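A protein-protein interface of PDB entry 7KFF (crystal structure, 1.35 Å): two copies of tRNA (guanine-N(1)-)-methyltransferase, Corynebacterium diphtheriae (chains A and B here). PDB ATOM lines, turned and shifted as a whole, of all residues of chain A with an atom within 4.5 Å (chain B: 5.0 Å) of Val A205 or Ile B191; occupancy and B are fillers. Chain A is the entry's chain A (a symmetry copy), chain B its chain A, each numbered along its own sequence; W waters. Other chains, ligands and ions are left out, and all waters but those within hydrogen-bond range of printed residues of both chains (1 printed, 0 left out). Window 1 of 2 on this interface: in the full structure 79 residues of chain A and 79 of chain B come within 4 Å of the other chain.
Hydrophobic or aromatic side chains of chain B that line the printed part of chain A: Phe B148, Ile B191, Tyr B194, Leu B196, Val B201 and Val B205.
Of the 12 printed residues of chain A, 6 touch a printed residue of chain B.
Hydrophobic or aromatic side chains of chain A that line the printed part of chain B: Ile A191, Tyr A194, Val A201, Leu A204 and Val A205.
Among the printed residues, no Asp or Glu carboxylate lies within 4 Å of a Lys or Arg side-chain nitrogen of the other chain.
Water W1 bridges OE2 of Glu A208 (2.7 Å) and N of Val B201 (2.9 Å).
Of chain B, only Ile B191, Tyr B194, Leu B196, Val B201 and Val B205 come within 4 Å of Val A205.
Ile B191 touches just these residues of chain A: Ile A191, Tyr A194 and Val A205.
Of the printed residues of chain A, Val B205 touches Ile A191 (3.8 Å), Tyr A194 (3.6 Å), Val A201 (3.7 Å) and Val A205 (3.6 Å).
Printed residues of chain B within 4 Å of Val A201: Val B205.
Gly B192 touches none of the printed residues of chain A.
Val B189 touches none of the printed residues of chain A.
The nearest residue of chain A that does not touch Ile B191 is Gly A192 (4.4 Å).
The nearest printed residue of chain B that does not touch Glu A208 is Ala B202 (6.5 Å).
Among the printed residues, pairs that only touch across the chains: Tyr A194 with Phe B148, Glu A208 with Leu B196, Val A205 with Val B205, Leu A204 with Val B201, Val A205 with Leu B196, Val A205 with Tyr B194, Tyr A194 with Val B205, Tyr A194 with Tyr B194, Val A205 with Val B201, Val A201 with Val B205, Glu A208 with Val B201, Ile A191 with Val B205 and Val A205 with Ile B191.
Ile B191 touches its own counterpart, Ile A191.
Ile A191 touches Tyr B194, and with the chains exchanged Tyr A194 touches Ile B191.
Ile A191 touches Val B205, and with the chains exchanged Val A205 touches Ile B191.
Tyr A194 touches its own counterpart, Tyr B194.
Of the 16 pairs that touch across the chains among the printed residues, 11 have their exchanged pair printed and touching as well.
The backbone carbonyl oxygen of Ile A191 lies close to the backbone carbonyl oxygen of Ile B191, at 3.2 Å.
The side-chain hydroxyl (OH) of Tyr B194 lies within hydrogen-bond range of the backbone carbonyl oxygen (O) of Ile A191, 2.8 Å away.
The backbone carbonyl oxygen of Ile B191 lies within hydrogen-bond range of the side-chain hydroxyl of Tyr A194 (2.8 Å).
The backbone NH (N) of Phe B148 lies within hydrogen-bond range of the backbone carbonyl oxygen (O) of Ser B190 (2.8 Å).
The backbone carbonyl oxygen of Ile B191 is in hydrogen-bond range of the side-chain hydroxyl of Tyr B194.
O of Ile A191 sits at hydrogen-bond distance from OH of Tyr A194 (3.2 Å).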
ATOM      1  N   ILE A 191     -13.720   3.580  14.557  1.00  0.00           N
ATOM      2  CA  ILE A 191     -12.480   2.807  14.682  1.00  0.00           C
ATOM      3  C   ILE A 191     -12.626   1.570  15.568  1.00  0.00           C
ATOM      4  O   ILE A 191     -11.694   0.751  15.632  1.00  0.00           O
ATOM      5  CB  ILE A 191     -11.244   3.664  15.050  1.00  0.00           C
ATOM      6  CG1 ILE A 191     -11.393   4.287  16.448  1.00  0.00           C
ATOM      7  CG2 ILE A 191     -10.991   4.694  13.967  1.00  0.00           C
ATOM      8  CD1 ILE A 191     -10.076   4.744  17.037  1.00  0.00           C
ATOM      9  N   GLY A 192     -13.766   1.394  16.227  1.00  0.00           N
ATOM     10  CA  GLY A 192     -13.990   0.213  17.041  1.00  0.00           C
ATOM     11  C   GLY A 192     -15.172   0.406  17.954  1.00  0.00           C
ATOM     12  O   GLY A 192     -15.715   1.512  18.081  1.00  0.00           O
ATOM     13  N   TYR A 194     -16.089   1.018  20.966  1.00  0.00           N
ATOM     14  CA  TYR A 194     -15.741   1.651  22.230  1.00  0.00           C
ATOM     15  C   TYR A 194     -15.934   3.142  22.006  1.00  0.00           C
ATOM     16  O   TYR A 194     -16.044   3.601  20.864  1.00  0.00           O
ATOM     17  CB  TYR A 194     -14.311   1.317  22.676  1.00  0.00           C
ATOM     18  CG  TYR A 194     -13.304   1.340  21.566  1.00  0.00           C
ATOM     19  CD1 TYR A 194     -12.783   2.536  21.107  1.00  0.00           C
ATOM     20  CD2 TYR A 194     -12.880   0.167  20.961  1.00  0.00           C
ATOM     21  CE1 TYR A 194     -11.868   2.570  20.062  1.00  0.00           C
ATOM     22  CE2 TYR A 194     -11.950   0.180  19.946  1.00  0.00           C
ATOM     23  CZ  TYR A 194     -11.448   1.395  19.501  1.00  0.00           C
ATOM     24  OH  TYR A 194     -10.543   1.451  18.480  1.00  0.00           O
ATOM     25  N   VAL A 201      -8.347  11.670  17.726  1.00  0.00           N
ATOM     26  CA  VAL A 201      -7.514  10.476  17.840  1.00  0.00           C
ATOM     27  C   VAL A 201      -7.851   9.479  16.743  1.00  0.00           C
ATOM     28  O   VAL A 201      -6.970   8.758  16.262  1.00  0.00           O
ATOM     29  CB  VAL A 201      -7.584   9.855  19.247  1.00  0.00           C
ATOM     30  CG1 VAL A 201      -8.921   9.165  19.514  1.00  0.00           C
ATOM     31  CG2 VAL A 201      -6.442   8.888  19.457  1.00  0.00           C
ATOM     32  N   ALA A 202      -9.112   9.426  16.324  1.00  0.00           N
ATOM     33  CA  ALA A 202      -9.476   8.537  15.227  1.00  0.00           C
ATOM     34  C   ALA A 202      -8.841   8.980  13.916  1.00  0.00           C
ATOM     35  O   ALA A 202      -8.498   8.130  13.091  1.00  0.00           O
ATOM     36  CB  ALA A 202     -10.994   8.490  15.097  1.00  0.00           C
ATOM     37  N   VAL A 203      -8.644  10.296  13.722  1.00  0.00           N
ATOM     38  CA  VAL A 203      -7.888  10.775  12.567  1.00  0.00           C
ATOM     39  C   VAL A 203      -6.468  10.223  12.600  1.00  0.00           C
ATOM     40  O   VAL A 203      -5.944   9.748  11.591  1.00  0.00           O
ATOM     41  CB  VAL A 203      -7.893  12.310  12.513  1.00  0.00           C
ATOM     42  CG1 VAL A 203      -7.013  12.765  11.357  1.00  0.00           C
ATOM     43  CG2 VAL A 203      -9.323  12.821  12.381  1.00  0.00           C
ATOM     44  N   LEU A 204      -5.820  10.287  13.763  1.00  0.00           N
ATOM     45  CA  LEU A 204      -4.461   9.763  13.854  1.00  0.00           C
ATOM     46  C   LEU A 204      -4.408   8.274  13.510  1.00  0.00           C
ATOM     47  O   LEU A 204      -3.479   7.820  12.832  1.00  0.00           O
ATOM     48  CB  LEU A 204      -3.907  10.006  15.260  1.00  0.00           C
ATOM     49  CG  LEU A 204      -3.775  11.466  15.724  1.00  0.00           C
ATOM     50  CD1 LEU A 204      -3.234  11.504  17.130  1.00  0.00           C
ATOM     51  CD2 LEU A 204      -2.899  12.249  14.779  1.00  0.00           C
ATOM     52  N   VAL A 205      -5.404   7.503  13.974  1.00  0.00           N
ATOM     53  CA  VAL A 205      -5.473   6.074  13.681  1.00  0.00           C
ATOM     54  C   VAL A 205      -5.600   5.841  12.188  1.00  0.00           C
ATOM     55  O   VAL A 205      -4.843   5.065  11.587  1.00  0.00           O
ATOM     56  CB  VAL A 205      -6.636   5.435  14.450  1.00  0.00           C
ATOM     57  CG1 VAL A 205      -6.929   4.047  13.910  1.00  0.00           C
ATOM     58  CG2 VAL A 205      -6.348   5.387  15.948  1.00  0.00           C
ATOM     59  N   ILE A 206      -6.579   6.487  11.567  1.00  0.00           N
ATOM     60  CA  ILE A 206      -6.837   6.273  10.145  1.00  0.00           C
ATOM     61  C   ILE A 206      -5.649   6.742   9.314  1.00  0.00           C
ATOM     62  O   ILE A 206      -5.229   6.074   8.357  1.00  0.00           O
ATOM     63  CB  ILE A 206      -8.152   6.962   9.743  1.00  0.00           C
ATOM     64  CG1 ILE A 206      -9.349   6.273  10.412  1.00  0.00           C
ATOM     65  CG2 ILE A 206      -8.303   6.960   8.238  1.00  0.00           C
ATOM     66  CD1 ILE A 206     -10.640   7.090  10.388  1.00  0.00           C
ATOM     67  N   ALA A 207      -5.069   7.880   9.690  1.00  0.00           N
ATOM     68  CA  ALA A 207      -3.915   8.388   8.962  1.00  0.00           C
ATOM     69  C   ALA A 207      -2.752   7.408   8.990  1.00  0.00           C
ATOM     70  O   ALA A 207      -2.099   7.198   7.962  1.00  0.00           O
ATOM     71  CB  ALA A 207      -3.517   9.759   9.496  1.00  0.00           C
ATOM     72  N   GLU A 208      -2.464   6.813  10.148  1.00  0.00           N
ATOM     73  CA  GLU A 208      -1.378   5.838  10.192  1.00  0.00           C
ATOM     74  C   GLU A 208      -1.651   4.678   9.245  1.00  0.00           C
ATOM     75  O   GLU A 208      -0.768   4.260   8.482  1.00  0.00           O
ATOM     76  CB  GLU A 208      -1.172   5.295  11.610  1.00  0.00           C
ATOM     77  CG  GLU A 208      -0.464   6.221  12.552  1.00  0.00           C
ATOM     78  CD  GLU A 208       0.367   5.518  13.615  1.00  0.00           C
ATOM     79  OE1 GLU A 208       0.349   4.260  13.718  1.00  0.00           O
ATOM     80  OE2 GLU A 208       1.037   6.253  14.361  1.00  0.00           O
ATOM     81  N   ALA A 209      -2.859   4.119   9.307  1.00  0.00           N
ATOM     82  CA  ALA A 209      -3.182   2.925   8.539  1.00  0.00           C
ATOM     83  C   ALA A 209      -3.205   3.194   7.044  1.00  0.00           C
ATOM     84  O   ALA A 209      -2.855   2.315   6.249  1.00  0.00           O
ATOM     85  CB  ALA A 209      -4.511   2.353   9.005  1.00  0.00           C
ATOM     86  N   PHE B 148      -9.928  -4.539  21.869  1.00  0.00           N
ATOM     87  CA  PHE B 148     -10.370  -3.569  22.864  1.00  0.00           C
ATOM     88  C   PHE B 148     -11.885  -3.402  22.777  1.00  0.00           C
ATOM     89  O   PHE B 148     -12.439  -3.158  21.696  1.00  0.00           O
ATOM     90  CB  PHE B 148      -9.686  -2.225  22.564  1.00  0.00           C
ATOM     91  CG  PHE B 148      -9.949  -1.135  23.578  1.00  0.00           C
ATOM     92  CD1 PHE B 148      -9.900  -1.389  24.947  1.00  0.00           C
ATOM     93  CD2 PHE B 148     -10.234   0.158  23.156  1.00  0.00           C
ATOM     94  CE1 PHE B 148     -10.119  -0.395  25.857  1.00  0.00           C
ATOM     95  CE2 PHE B 148     -10.460   1.155  24.082  1.00  0.00           C
ATOM     96  CZ  PHE B 148     -10.406   0.884  25.412  1.00  0.00           C
ATOM     97  N   VAL B 189      -3.549  -6.156  23.287  1.00  0.00           N
ATOM     98  CA  VAL B 189      -4.820  -5.537  22.928  1.00  0.00           C
ATOM     99  C   VAL B 189      -4.738  -4.916  21.538  1.00  0.00           C
ATOM    100  O   VAL B 189      -3.836  -4.119  21.255  1.00  0.00           O
ATOM    101  CB  VAL B 189      -5.261  -4.499  23.985  1.00  0.00           C
ATOM    102  CG1 VAL B 189      -4.161  -3.507  24.319  1.00  0.00           C
ATOM    103  CG2 VAL B 189      -6.526  -3.774  23.555  1.00  0.00           C
ATOM    104  N   SER B 190      -5.692  -5.269  20.688  1.00  0.00           N
ATOM    105  CA  SER B 190      -5.838  -4.648  19.386  1.00  0.00           C
ATOM    106  C   SER B 190      -6.957  -3.616  19.429  1.00  0.00           C
ATOM    107  O   SER B 190      -8.030  -3.879  19.977  1.00  0.00           O
ATOM    108  CB  SER B 190      -6.215  -5.687  18.335  1.00  0.00           C
ATOM    109  OG  SER B 190      -6.439  -4.992  17.117  1.00  0.00           O
ATOM    110  N   ILE B 191      -6.736  -2.454  18.807  1.00  0.00           N
ATOM    111  CA  ILE B 191      -7.823  -1.472  18.728  1.00  0.00           C
ATOM    112  C   ILE B 191      -8.751  -1.695  17.533  1.00  0.00           C
ATOM    113  O   ILE B 191      -9.795  -1.027  17.439  1.00  0.00           O
ATOM    114  CB  ILE B 191      -7.347  -0.003  18.848  1.00  0.00           C
ATOM    115  CG1 ILE B 191      -6.449   0.393  17.665  1.00  0.00           C
ATOM    116  CG2 ILE B 191      -6.682   0.214  20.193  1.00  0.00           C
ATOM    117  CD1 ILE B 191      -6.327   1.891  17.486  1.00  0.00           C
ATOM    118  N   GLY B 192      -8.425  -2.623  16.642  1.00  0.00           N
ATOM    119  CA  GLY B 192      -9.291  -2.925  15.517  1.00  0.00           C
ATOM    120  C   GLY B 192      -8.560  -3.729  14.476  1.00  0.00           C
ATOM    121  O   GLY B 192      -7.336  -3.911  14.543  1.00  0.00           O
ATOM    122  N   ASP B 193      -9.323  -4.178  13.478  1.00  0.00           N
ATOM    123  CA  ASP B 193      -8.801  -5.101  12.463  1.00  0.00           C
ATOM    124  C   ASP B 193      -8.198  -4.310  11.299  1.00  0.00           C
ATOM    125  O   ASP B 193      -8.666  -4.317  10.159  1.00  0.00           O
ATOM    126  CB  ASP B 193      -9.880  -6.073  11.988  1.00  0.00           C
ATOM    127  CG  ASP B 193     -10.279  -7.111  13.042  1.00  0.00           C
ATOM    128  OD1 ASP B 193      -9.697  -7.157  14.149  1.00  0.00           O
ATOM    129  OD2 ASP B 193     -11.180  -7.923  12.731  1.00  0.00           O
ATOM    130  N   TYR B 194      -7.113  -3.621  11.615  1.00  0.00           N
ATOM    131  CA  TYR B 194      -6.389  -2.798  10.657  1.00  0.00           C
ATOM    132  C   TYR B 194      -4.987  -2.646  11.226  1.00  0.00           C
ATOM    133  O   TYR B 194      -4.749  -2.932  12.406  1.00  0.00           O
ATOM    134  CB  TYR B 194      -7.064  -1.440  10.427  1.00  0.00           C
ATOM    135  CG  TYR B 194      -7.580  -0.793  11.677  1.00  0.00           C
ATOM    136  CD1 TYR B 194      -6.724  -0.119  12.529  1.00  0.00           C
ATOM    137  CD2 TYR B 194      -8.920  -0.867  12.020  1.00  0.00           C
ATOM    138  CE1 TYR B 194      -7.186   0.463  13.704  1.00  0.00           C
ATOM    139  CE2 TYR B 194      -9.401  -0.269  13.164  1.00  0.00           C
ATOM    140  CZ  TYR B 194      -8.520   0.397  14.005  1.00  0.00           C
ATOM    141  OH  TYR B 194      -8.954   0.980  15.160  1.00  0.00           O
ATOM    142  N   LEU B 196      -1.630  -0.517  12.043  1.00  0.00           N
ATOM    143  CA  LEU B 196      -1.044   0.771  12.344  1.00  0.00           C
ATOM    144  C   LEU B 196       0.471   0.715  12.203  1.00  0.00           C
ATOM    145  O   LEU B 196       1.060  -0.344  11.976  1.00  0.00           O
ATOM    146  CB  LEU B 196      -1.373   1.171  13.780  1.00  0.00           C
ATOM    147  CG  LEU B 196      -2.872   1.131  14.076  1.00  0.00           C
ATOM    148  CD1 LEU B 196      -3.106   1.324  15.558  1.00  0.00           C
ATOM    149  CD2 LEU B 196      -3.633   2.132  13.226  1.00  0.00           C
ATOM    150  N   VAL B 201      -0.313   5.488  19.011  1.00  0.00           N
ATOM    151  CA  VAL B 201      -1.663   5.978  18.749  1.00  0.00           C
ATOM    152  C   VAL B 201      -2.696   5.115  19.453  1.00  0.00           C
ATOM    153  O   VAL B 201      -3.738   5.615  19.890  1.00  0.00           O
ATOM    154  CB  VAL B 201      -1.942   6.125  17.242  1.00  0.00           C
ATOM    155  CG1 VAL B 201      -2.107   4.774  16.546  1.00  0.00           C
ATOM    156  CG2 VAL B 201      -3.161   6.988  17.009  1.00  0.00           C
ATOM    157  N   ALA B 202      -2.427   3.819  19.590  1.00  0.00           N
ATOM    158  CA  ALA B 202      -3.350   2.958  20.319  1.00  0.00           C
ATOM    159  C   ALA B 202      -3.396   3.315  21.799  1.00  0.00           C
ATOM    160  O   ALA B 202      -4.454   3.193  22.419  1.00  0.00           O
ATOM    161  CB  ALA B 202      -2.938   1.503  20.133  1.00  0.00           C
ATOM    162  N   VAL B 205      -5.846   6.134  22.023  1.00  0.00           N
ATOM    163  CA  VAL B 205      -7.206   5.620  21.907  1.00  0.00           C
ATOM    164  C   VAL B 205      -7.674   5.045  23.230  1.00  0.00           C
ATOM    165  O   VAL B 205      -8.752   5.386  23.739  1.00  0.00           O
ATOM    166  CB  VAL B 205      -7.280   4.577  20.783  1.00  0.00           C
ATOM    167  CG1 VAL B 205      -8.582   3.799  20.868  1.00  0.00           C
ATOM    168  CG2 VAL B 205      -7.125   5.230  19.412  1.00  0.00           C
ATOM    169  N   ILE B 206      -6.886   4.140  23.797  1.00  0.00           N
ATOM    170  CA  ILE B 206      -7.280   3.468  25.032  1.00  0.00           C
ATOM    171  C   ILE B 206      -7.384   4.472  26.173  1.00  0.00           C
ATOM    172  O   ILE B 206      -8.323   4.434  26.980  1.00  0.00           O
ATOM    173  CB  ILE B 206      -6.302   2.321  25.337  1.00  0.00           C
ATOM    174  CG1 ILE B 206      -6.432   1.208  24.290  1.00  0.00           C
ATOM    175  CG2 ILE B 206      -6.550   1.781  26.728  1.00  0.00           C
ATOM    176  CD1 ILE B 206      -5.269   0.216  24.277  1.00  0.00           C
HETATM  177  O   HOH W   1       1.423   5.023  16.738  1.00  0.00           O
